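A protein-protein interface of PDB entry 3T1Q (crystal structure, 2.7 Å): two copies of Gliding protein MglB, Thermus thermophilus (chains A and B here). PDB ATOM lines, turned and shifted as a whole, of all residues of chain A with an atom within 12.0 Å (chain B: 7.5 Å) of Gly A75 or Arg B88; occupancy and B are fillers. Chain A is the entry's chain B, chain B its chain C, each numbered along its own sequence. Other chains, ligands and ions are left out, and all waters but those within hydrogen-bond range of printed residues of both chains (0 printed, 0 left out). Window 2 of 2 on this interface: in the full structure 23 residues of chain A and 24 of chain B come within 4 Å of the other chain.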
ATOM      1  N   ALA A  66       0.420  12.362 -29.169  1.00  0.00           N
ATOM      2  CA  ALA A  66      -0.874  12.759 -28.625  1.00  0.00           C
ATOM      3  C   ALA A  66      -0.884  12.607 -27.097  1.00  0.00           C
ATOM      4  O   ALA A  66      -1.209  13.563 -26.369  1.00  0.00           O
ATOM      5  CB  ALA A  66      -2.021  11.966 -29.277  1.00  0.00           C
ATOM      6  N   THR A  67      -0.512  11.423 -26.607  1.00  0.00           N
ATOM      7  CA  THR A  67      -0.505  11.181 -25.176  1.00  0.00           C
ATOM      8  C   THR A  67       0.501  12.023 -24.412  1.00  0.00           C
ATOM      9  O   THR A  67       0.159  12.401 -23.287  1.00  0.00           O
ATOM     10  CB  THR A  67      -0.382   9.709 -24.805  1.00  0.00           C
ATOM     11  OG1 THR A  67       0.870   9.222 -25.231  1.00  0.00           O
ATOM     12  CG2 THR A  67      -1.451   8.909 -25.513  1.00  0.00           C
ATOM     13  N   GLN A  68       1.700  12.344 -24.951  1.00  0.00           N
ATOM     14  CA  GLN A  68       2.570  13.333 -24.280  1.00  0.00           C
ATOM     15  C   GLN A  68       1.835  14.666 -24.207  1.00  0.00           C
ATOM     16  O   GLN A  68       1.905  15.371 -23.198  1.00  0.00           O
ATOM     17  CB  GLN A  68       3.915  13.522 -24.996  1.00  0.00           C
ATOM     18  CG  GLN A  68       4.689  14.760 -24.572  1.00  0.00           C
ATOM     19  CD  GLN A  68       5.724  14.471 -23.488  1.00  0.00           C
ATOM     20  OE1 GLN A  68       5.478  14.671 -22.268  1.00  0.00           O
ATOM     21  NE2 GLN A  68       6.894  13.977 -23.928  1.00  0.00           N
ATOM     22  N   ALA A  69       1.124  15.012 -25.287  1.00  0.00           N
ATOM     23  CA  ALA A  69       0.427  16.286 -25.286  1.00  0.00           C
ATOM     24  C   ALA A  69      -0.717  16.311 -24.272  1.00  0.00           C
ATOM     25  O   ALA A  69      -0.988  17.381 -23.726  1.00  0.00           O
ATOM     26  CB  ALA A  69      -0.018  16.711 -26.674  1.00  0.00           C
ATOM     27  N   LEU A  70      -1.369  15.171 -24.004  1.00  0.00           N
ATOM     28  CA  LEU A  70      -2.442  15.129 -22.991  1.00  0.00           C
ATOM     29  C   LEU A  70      -1.889  15.290 -21.581  1.00  0.00           C
ATOM     30  O   LEU A  70      -2.428  16.067 -20.768  1.00  0.00           O
ATOM     31  CB  LEU A  70      -3.270  13.854 -23.047  1.00  0.00           C
ATOM     32  CG  LEU A  70      -4.296  13.842 -24.170  1.00  0.00           C
ATOM     33  CD1 LEU A  70      -4.555  12.404 -24.639  1.00  0.00           C
ATOM     34  CD2 LEU A  70      -5.608  14.599 -23.773  1.00  0.00           C
ATOM     35  N   ALA A  71      -0.808  14.557 -21.312  1.00  0.00           N
ATOM     36  CA  ALA A  71      -0.036  14.726 -20.104  1.00  0.00           C
ATOM     37  C   ALA A  71       0.299  16.198 -19.827  1.00  0.00           C
ATOM     38  O   ALA A  71      -0.029  16.724 -18.753  1.00  0.00           O
ATOM     39  CB  ALA A  71       1.242  13.890 -20.190  1.00  0.00           C
ATOM     40  N   LYS A  72       0.953  16.857 -20.781  1.00  0.00           N
ATOM     41  CA  LYS A  72       1.379  18.243 -20.591  1.00  0.00           C
ATOM     42  C   LYS A  72       0.132  19.091 -20.278  1.00  0.00           C
ATOM     43  O   LYS A  72       0.137  19.927 -19.374  1.00  0.00           O
ATOM     44  CB  LYS A  72       2.145  18.753 -21.812  1.00  0.00           C
ATOM     45  CG  LYS A  72       2.876  20.093 -21.687  1.00  0.00           C
ATOM     46  CD  LYS A  72       2.710  20.859 -23.047  1.00  0.00           C
ATOM     47  CE  LYS A  72       3.095  22.349 -23.034  1.00  0.00           C
ATOM     48  NZ  LYS A  72       4.542  22.410 -22.754  1.00  0.00           N
ATOM     49  N   LEU A  73      -0.972  18.798 -20.943  1.00  0.00           N
ATOM     50  CA  LEU A  73      -2.180  19.559 -20.735  1.00  0.00           C
ATOM     51  C   LEU A  73      -2.820  19.377 -19.358  1.00  0.00           C
ATOM     52  O   LEU A  73      -3.731  20.141 -19.002  1.00  0.00           O
ATOM     53  CB  LEU A  73      -3.201  19.219 -21.814  1.00  0.00           C
ATOM     54  CG  LEU A  73      -4.431  20.122 -21.797  1.00  0.00           C
ATOM     55  CD1 LEU A  73      -4.120  21.430 -22.545  1.00  0.00           C
ATOM     56  CD2 LEU A  73      -5.582  19.349 -22.405  1.00  0.00           C
ATOM     57  N   LEU A  74      -2.391  18.361 -18.621  1.00  0.00           N
ATOM     58  CA  LEU A  74      -2.853  18.140 -17.275  1.00  0.00           C
ATOM     59  C   LEU A  74      -1.750  18.411 -16.243  1.00  0.00           C
ATOM     60  O   LEU A  74      -1.774  17.904 -15.124  1.00  0.00           O
ATOM     61  CB  LEU A  74      -3.384  16.718 -17.160  1.00  0.00           C
ATOM     62  CG  LEU A  74      -4.482  16.438 -18.168  1.00  0.00           C
ATOM     63  CD1 LEU A  74      -5.070  15.092 -17.993  1.00  0.00           C
ATOM     64  CD2 LEU A  74      -5.574  17.444 -18.039  1.00  0.00           C
ATOM     65  N   GLY A  75      -0.761  19.203 -16.621  1.00  0.00           N
ATOM     66  CA  GLY A  75       0.361  19.459 -15.716  1.00  0.00           C
ATOM     67  C   GLY A  75       1.213  18.237 -15.340  1.00  0.00           C
ATOM     68  O   GLY A  75       1.780  18.196 -14.242  1.00  0.00           O
ATOM     69  N   GLU A  76       1.319  17.259 -16.247  1.00  0.00           N
ATOM     70  CA  GLU A  76       2.070  16.013 -15.989  1.00  0.00           C
ATOM     71  C   GLU A  76       3.237  15.901 -16.912  1.00  0.00           C
ATOM     72  O   GLU A  76       3.202  16.346 -18.043  1.00  0.00           O
ATOM     73  CB  GLU A  76       1.186  14.766 -16.108  1.00  0.00           C
ATOM     74  CG  GLU A  76       0.139  14.602 -14.963  1.00  0.00           C
ATOM     75  CD  GLU A  76       0.704  14.083 -13.608  1.00  0.00           C
ATOM     76  OE1 GLU A  76      -0.105  13.889 -12.665  1.00  0.00           O
ATOM     77  OE2 GLU A  76       1.939  13.862 -13.479  1.00  0.00           O
ATOM     78  N   ALA A  77       4.301  15.320 -16.407  1.00  0.00           N
ATOM     79  CA  ALA A  77       5.507  15.066 -17.216  1.00  0.00           C
ATOM     80  C   ALA A  77       5.258  14.007 -18.300  1.00  0.00           C
ATOM     81  O   ALA A  77       5.707  14.171 -19.424  1.00  0.00           O
ATOM     82  CB  ALA A  77       6.669  14.633 -16.284  1.00  0.00           C
ATOM     83  N   ARG A  78       4.525  12.948 -17.932  1.00  0.00           N
ATOM     84  CA  ARG A  78       4.273  11.772 -18.747  1.00  0.00           C
ATOM     85  C   ARG A  78       3.221  10.896 -18.075  1.00  0.00           C
ATOM     86  O   ARG A  78       3.012  10.998 -16.868  1.00  0.00           O
ATOM     87  CB  ARG A  78       5.568  10.962 -18.925  1.00  0.00           C
ATOM     88  CG  ARG A  78       6.110  10.211 -17.685  1.00  0.00           C
ATOM     89  CD  ARG A  78       7.509   9.648 -17.960  1.00  0.00           C
ATOM     90  NE  ARG A  78       8.547  10.641 -17.639  1.00  0.00           N
ATOM     91  CZ  ARG A  78       9.167  11.435 -18.524  1.00  0.00           C
ATOM     92  NH1 ARG A  78       8.875  11.365 -19.827  1.00  0.00           N
ATOM     93  NH2 ARG A  78      10.086  12.303 -18.109  1.00  0.00           N
ATOM     94  N   PHE A  79       2.552  10.033 -18.836  1.00  0.00           N
ATOM     95  CA  PHE A  79       1.829   8.958 -18.191  1.00  0.00           C
ATOM     96  C   PHE A  79       2.805   7.813 -18.140  1.00  0.00           C
ATOM     97  O   PHE A  79       3.960   7.971 -18.520  1.00  0.00           O
ATOM     98  CB  PHE A  79       0.581   8.570 -18.958  1.00  0.00           C
ATOM     99  CG  PHE A  79      -0.393   9.702 -19.151  1.00  0.00           C
ATOM    100  CD1 PHE A  79      -1.013  10.298 -18.064  1.00  0.00           C
ATOM    101  CD2 PHE A  79      -0.686  10.175 -20.425  1.00  0.00           C
ATOM    102  CE1 PHE A  79      -1.897  11.337 -18.239  1.00  0.00           C
ATOM    103  CE2 PHE A  79      -1.578  11.204 -20.605  1.00  0.00           C
ATOM    104  CZ  PHE A  79      -2.182  11.793 -19.509  1.00  0.00           C
ATOM    105  N   GLN A  80       2.383   6.654 -17.666  1.00  0.00           N
ATOM    106  CA  GLN A  80       3.333   5.547 -17.635  1.00  0.00           C
ATOM    107  C   GLN A  80       3.374   4.697 -18.924  1.00  0.00           C
ATOM    108  O   GLN A  80       2.834   5.103 -19.952  1.00  0.00           O
ATOM    109  CB  GLN A  80       3.118   4.694 -16.392  1.00  0.00           C
ATOM    110  CG  GLN A  80       1.773   4.043 -16.266  1.00  0.00           C
ATOM    111  CD  GLN A  80       1.379   4.043 -14.831  1.00  0.00           C
ATOM    112  OE1 GLN A  80       1.850   4.906 -14.079  1.00  0.00           O
ATOM    113  NE2 GLN A  80       0.531   3.087 -14.415  1.00  0.00           N
ATOM    114  N   ARG B  27     -13.265  14.845 -12.085  1.00  0.00           N
ATOM    115  CA  ARG B  27     -13.416  16.302 -12.280  1.00  0.00           C
ATOM    116  C   ARG B  27     -14.289  16.692 -13.508  1.00  0.00           C
ATOM    117  O   ARG B  27     -15.227  17.493 -13.385  1.00  0.00           O
ATOM    118  CB  ARG B  27     -12.074  16.969 -12.468  1.00  0.00           C
ATOM    119  CG  ARG B  27     -11.216  17.071 -11.273  1.00  0.00           C
ATOM    120  CD  ARG B  27     -10.175  18.143 -11.512  1.00  0.00           C
ATOM    121  NE  ARG B  27      -9.276  18.151 -10.375  1.00  0.00           N
ATOM    122  CZ  ARG B  27      -8.116  18.804 -10.292  1.00  0.00           C
ATOM    123  NH1 ARG B  27      -7.655  19.531 -11.300  1.00  0.00           N
ATOM    124  NH2 ARG B  27      -7.403  18.697  -9.178  1.00  0.00           N
ATOM    125  N   PRO B  51      -8.956  22.488 -18.482  1.00  0.00           N
ATOM    126  CA  PRO B  51      -8.162  22.974 -19.609  1.00  0.00           C
ATOM    127  C   PRO B  51      -9.030  23.044 -20.910  1.00  0.00           C
ATOM    128  O   PRO B  51     -10.167  22.526 -20.931  1.00  0.00           O
ATOM    129  CB  PRO B  51      -7.035  21.943 -19.678  1.00  0.00           C
ATOM    130  CG  PRO B  51      -7.617  20.676 -19.125  1.00  0.00           C
ATOM    131  CD  PRO B  51      -8.569  21.123 -18.062  1.00  0.00           C
ATOM    132  N   GLN B  85      -2.401   7.390 -16.654  1.00  0.00           N
ATOM    133  CA  GLN B  85      -2.130   7.628 -15.245  1.00  0.00           C
ATOM    134  C   GLN B  85      -0.851   8.421 -15.019  1.00  0.00           C
ATOM    135  O   GLN B  85       0.241   7.956 -15.293  1.00  0.00           O
ATOM    136  CB  GLN B  85      -1.956   6.273 -14.590  1.00  0.00           C
ATOM    137  CG  GLN B  85      -1.801   6.319 -13.098  1.00  0.00           C
ATOM    138  CD  GLN B  85      -3.133   6.180 -12.401  1.00  0.00           C
ATOM    139  OE1 GLN B  85      -3.704   5.067 -12.368  1.00  0.00           O
ATOM    140  NE2 GLN B  85      -3.647   7.300 -11.841  1.00  0.00           N
ATOM    141  N   GLY B  86      -0.988   9.623 -14.497  1.00  0.00           N
ATOM    142  CA  GLY B  86       0.173  10.395 -14.035  1.00  0.00           C
ATOM    143  C   GLY B  86       0.368  10.245 -12.533  1.00  0.00           C
ATOM    144  O   GLY B  86      -0.290   9.399 -11.896  1.00  0.00           O
ATOM    145  N   GLU B  87       1.274  11.056 -11.985  1.00  0.00           N
ATOM    146  CA  GLU B  87       1.534  11.086 -10.539  1.00  0.00           C
ATOM    147  C   GLU B  87       0.257  11.518  -9.780  1.00  0.00           C
ATOM    148  O   GLU B  87      -0.026  10.992  -8.699  1.00  0.00           O
ATOM    149  CB  GLU B  87       2.705  12.026 -10.148  1.00  0.00           C
ATOM    150  CG  GLU B  87       4.105  11.780 -10.772  1.00  0.00           C
ATOM    151  CD  GLU B  87       4.924  10.662 -10.054  1.00  0.00           C
ATOM    152  OE1 GLU B  87       6.007  10.999  -9.463  1.00  0.00           O
ATOM    153  OE2 GLU B  87       4.492   9.458 -10.097  1.00  0.00           O
ATOM    154  N   ARG B  88      -0.511  12.458 -10.352  1.00  0.00           N
ATOM    155  CA  ARG B  88      -1.754  12.948  -9.708  1.00  0.00           C
ATOM    156  C   ARG B  88      -2.999  12.813 -10.612  1.00  0.00           C
ATOM    157  O   ARG B  88      -3.989  12.188 -10.230  1.00  0.00           O
ATOM    158  CB  ARG B  88      -1.592  14.412  -9.224  1.00  0.00           C
ATOM    159  CG  ARG B  88      -0.385  14.692  -8.278  1.00  0.00           C
ATOM    160  CD  ARG B  88       0.123  16.138  -8.389  1.00  0.00           C
ATOM    161  NE  ARG B  88       0.732  16.484  -9.697  1.00  0.00           N
ATOM    162  CZ  ARG B  88       2.032  16.353 -10.033  1.00  0.00           C
ATOM    163  NH1 ARG B  88       2.926  15.832  -9.165  1.00  0.00           N
ATOM    164  NH2 ARG B  88       2.441  16.730 -11.258  1.00  0.00           N
ATOM    165  N   MET B  89      -2.917  13.408 -11.808  1.00  0.00           N
ATOM    166  CA  MET B  89      -3.981  13.446 -12.821  1.00  0.00           C
ATOM    167  C   MET B  89      -4.135  12.157 -13.673  1.00  0.00           C
ATOM    168  O   MET B  89      -3.151  11.479 -13.956  1.00  0.00           O
ATOM    169  CB  MET B  89      -3.686  14.628 -13.748  1.00  0.00           C
ATOM    170  CG  MET B  89      -3.696  16.009 -13.079  1.00  0.00           C
ATOM    171  SD  MET B  89      -5.144  16.308 -12.051  1.00  0.00           S
ATOM    172  CE  MET B  89      -6.529  16.174 -13.200  1.00  0.00           C
ATOM    173  N   GLY B  90      -5.359  11.827 -14.092  1.00  0.00           N
ATOM    174  CA  GLY B  90      -5.593  10.669 -15.005  1.00  0.00           C
ATOM    175  C   GLY B  90      -6.774  10.818 -15.978  1.00  0.00           C
ATOM    176  O   GLY B  90      -7.662  11.655 -15.760  1.00  0.00           O
ATOM    177  N   PHE B 106      -9.802  12.822 -14.120  1.00  0.00           N
ATOM    178  CA  PHE B 106      -9.808  12.654 -12.680  1.00  0.00           C
ATOM    179  C   PHE B 106      -8.469  12.923 -12.033  1.00  0.00           C
ATOM    180  O   PHE B 106      -7.456  13.027 -12.724  1.00  0.00           O
ATOM    181  CB  PHE B 106     -10.309  11.257 -12.304  1.00  0.00           C
ATOM    182  CG  PHE B 106      -9.461  10.123 -12.844  1.00  0.00           C
ATOM    183  CD1 PHE B 106      -8.463   9.531 -12.044  1.00  0.00           C
ATOM    184  CD2 PHE B 106      -9.692   9.609 -14.126  1.00  0.00           C
ATOM    185  CE1 PHE B 106      -7.667   8.456 -12.526  1.00  0.00           C
ATOM    186  CE2 PHE B 106      -8.924   8.534 -14.622  1.00  0.00           C
ATOM    187  CZ  PHE B 106      -7.895   7.966 -13.818  1.00  0.00           C
ATOM    188  N   ASP B 107      -8.475  13.025 -10.700  1.00  0.00           N
ATOM    189  CA  ASP B 107      -7.275  13.357  -9.914  1.00  0.00           C
ATOM    190  C   ASP B 107      -7.040  12.370  -8.780  1.00  0.00           C
ATOM    191  O   ASP B 107      -7.694  11.298  -8.716  1.00  0.00           O
ATOM    192  CB  ASP B 107      -7.318  14.793  -9.393  1.00  0.00           C
ATOM    193  CG  ASP B 107      -8.476  15.049  -8.421  1.00  0.00           C
ATOM    194  OD1 ASP B 107      -8.743  16.233  -8.102  1.00  0.00           O
ATOM    195  OD2 ASP B 107      -9.123  14.082  -7.973  1.00  0.00           O
ATOM    196  N   GLU B 108      -6.089  12.720  -7.904  1.00  0.00           N
ATOM    197  CA  GLU B 108      -5.718  11.834  -6.775  1.00  0.00           C
ATOM    198  C   GLU B 108      -6.862  11.557  -5.763  1.00  0.00           C
ATOM    199  O   GLU B 108      -6.788  10.611  -5.016  1.00  0.00           O
ATOM    200  CB  GLU B 108      -4.460  12.327  -6.068  1.00  0.00           C
ATOM    201  CG  GLU B 108      -4.643  13.597  -5.214  1.00  0.00           C
ATOM    202  CD  GLU B 108      -4.705  14.879  -6.049  1.00  0.00           C
ATOM    203  OE1 GLU B 108      -4.217  14.880  -7.226  1.00  0.00           O
ATOM    204  OE2 GLU B 108      -5.245  15.891  -5.518  1.00  0.00           O
ATOM    205  N   THR B 109      -7.920  12.361  -5.780  1.00  0.00           N
ATOM    206  CA  THR B 109      -9.009  12.194  -4.839  1.00  0.00           C
ATOM    207  C   THR B 109     -10.003  11.102  -5.245  1.00  0.00           C
ATOM    208  O   THR B 109     -10.767  10.605  -4.396  1.00  0.00           O
ATOM    209  CB  THR B 109      -9.787  13.523  -4.581  1.00  0.00           C
ATOM    210  OG1 THR B 109     -10.532  13.925  -5.755  1.00  0.00           O
ATOM    211  CG2 THR B 109      -8.832  14.662  -4.064  1.00  0.00           C
ATOM    212  N   ALA B 110      -9.992  10.743  -6.536  1.00  0.00           N
ATOM    213  CA  ALA B 110     -10.952   9.787  -7.092  1.00  0.00           C
ATOM    214  C   ALA B 110     -10.440   8.330  -7.124  1.00  0.00           C
ATOM    215  O   ALA B 110      -9.463   8.016  -7.800  1.00  0.00           O
ATOM    216  CB  ALA B 110     -11.379  10.225  -8.474  1.00  0.00           C
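O of Ala A71 is in hydrogen-bond range of N of Glu A76 (2.9 Å).
O of Arg B88 is in hydrogen-bond range of N of Glu B108 (3.2 Å).
No position is printed for both chains.
NH2 of Arg B88 lies within salt-bridge range of OE2 of Glu A76.
The side-chain carboxylate (OE1) of Glu A76 sits at hydrogen-bond distance from the backbone NH (N) of Met B89 (3.0 Å).
OE1 of Glu A76 lies within hydrogen-bond range of N of Glu B87, at 3.2 Å.
The backbone NH of Gln A80 sits at hydrogen-bond distance from the backbone carbonyl oxygen of Gln B85 (3.5 Å).
The guanidinium group (NH2) of Arg B88 lies within hydrogen-bond range of the backbone carbonyl oxygen (O) of Gly A75 (3.4 Å).
Leu A73 touches Pro B51.
Leu A74 touches Pro B51 (CD2 to CG, 3.97 Å).
Met B89 touches Leu A74 (CG to O, 3.4 Å).
Gly B86 touches Glu A76 (C to OE1, 3.7 Å).
Phe A79 touches Gln B85.
Phe A79 touches Gly B86.
Of the printed residues of chain B, Leu A73 touches Pro B51.
Gly A75 touches just one residue of chain B: Arg B88.
Of the printed residues of chain B, Phe A79 touches Gln B85 (3.5 Å) and Gly B86 (3.6 Å).
Of the printed residues of chain B, Gln A80 touches Gln B85 (3.5 Å).
Printed residues of chain A within 4 Å of Gln B85: Phe A79 and Gln A80.
Of chain A, only Glu A76 (3.2 Å) comes within 4 Å of Glu B87.
Arg B88 touches just these residues of chain A: Gly A75 and Glu A76.
Met B89 touches just these residues of chain A: Leu A74 and Glu A76.
No residue of chain A comes within 4 Å of Phe B106.
No residue of chain A comes within 4 Å of Glu B108.
The nearest printed residue of chain B that does not touch Gln A80 is Gly B86 (5.4 Å).
Hydrophobic or aromatic side chains of chain A that line the printed part of chain B: Leu A73, Leu A74 and Phe A79.
Printed residues of chain B that touch a printed residue of chain A: Pro B51, Gln B85, Gly B86, Glu B87, Arg B88 and Met B89.
Hydrophobic or aromatic side chains of chain B that line the printed part of chain A: Pro B51 and Met B89.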
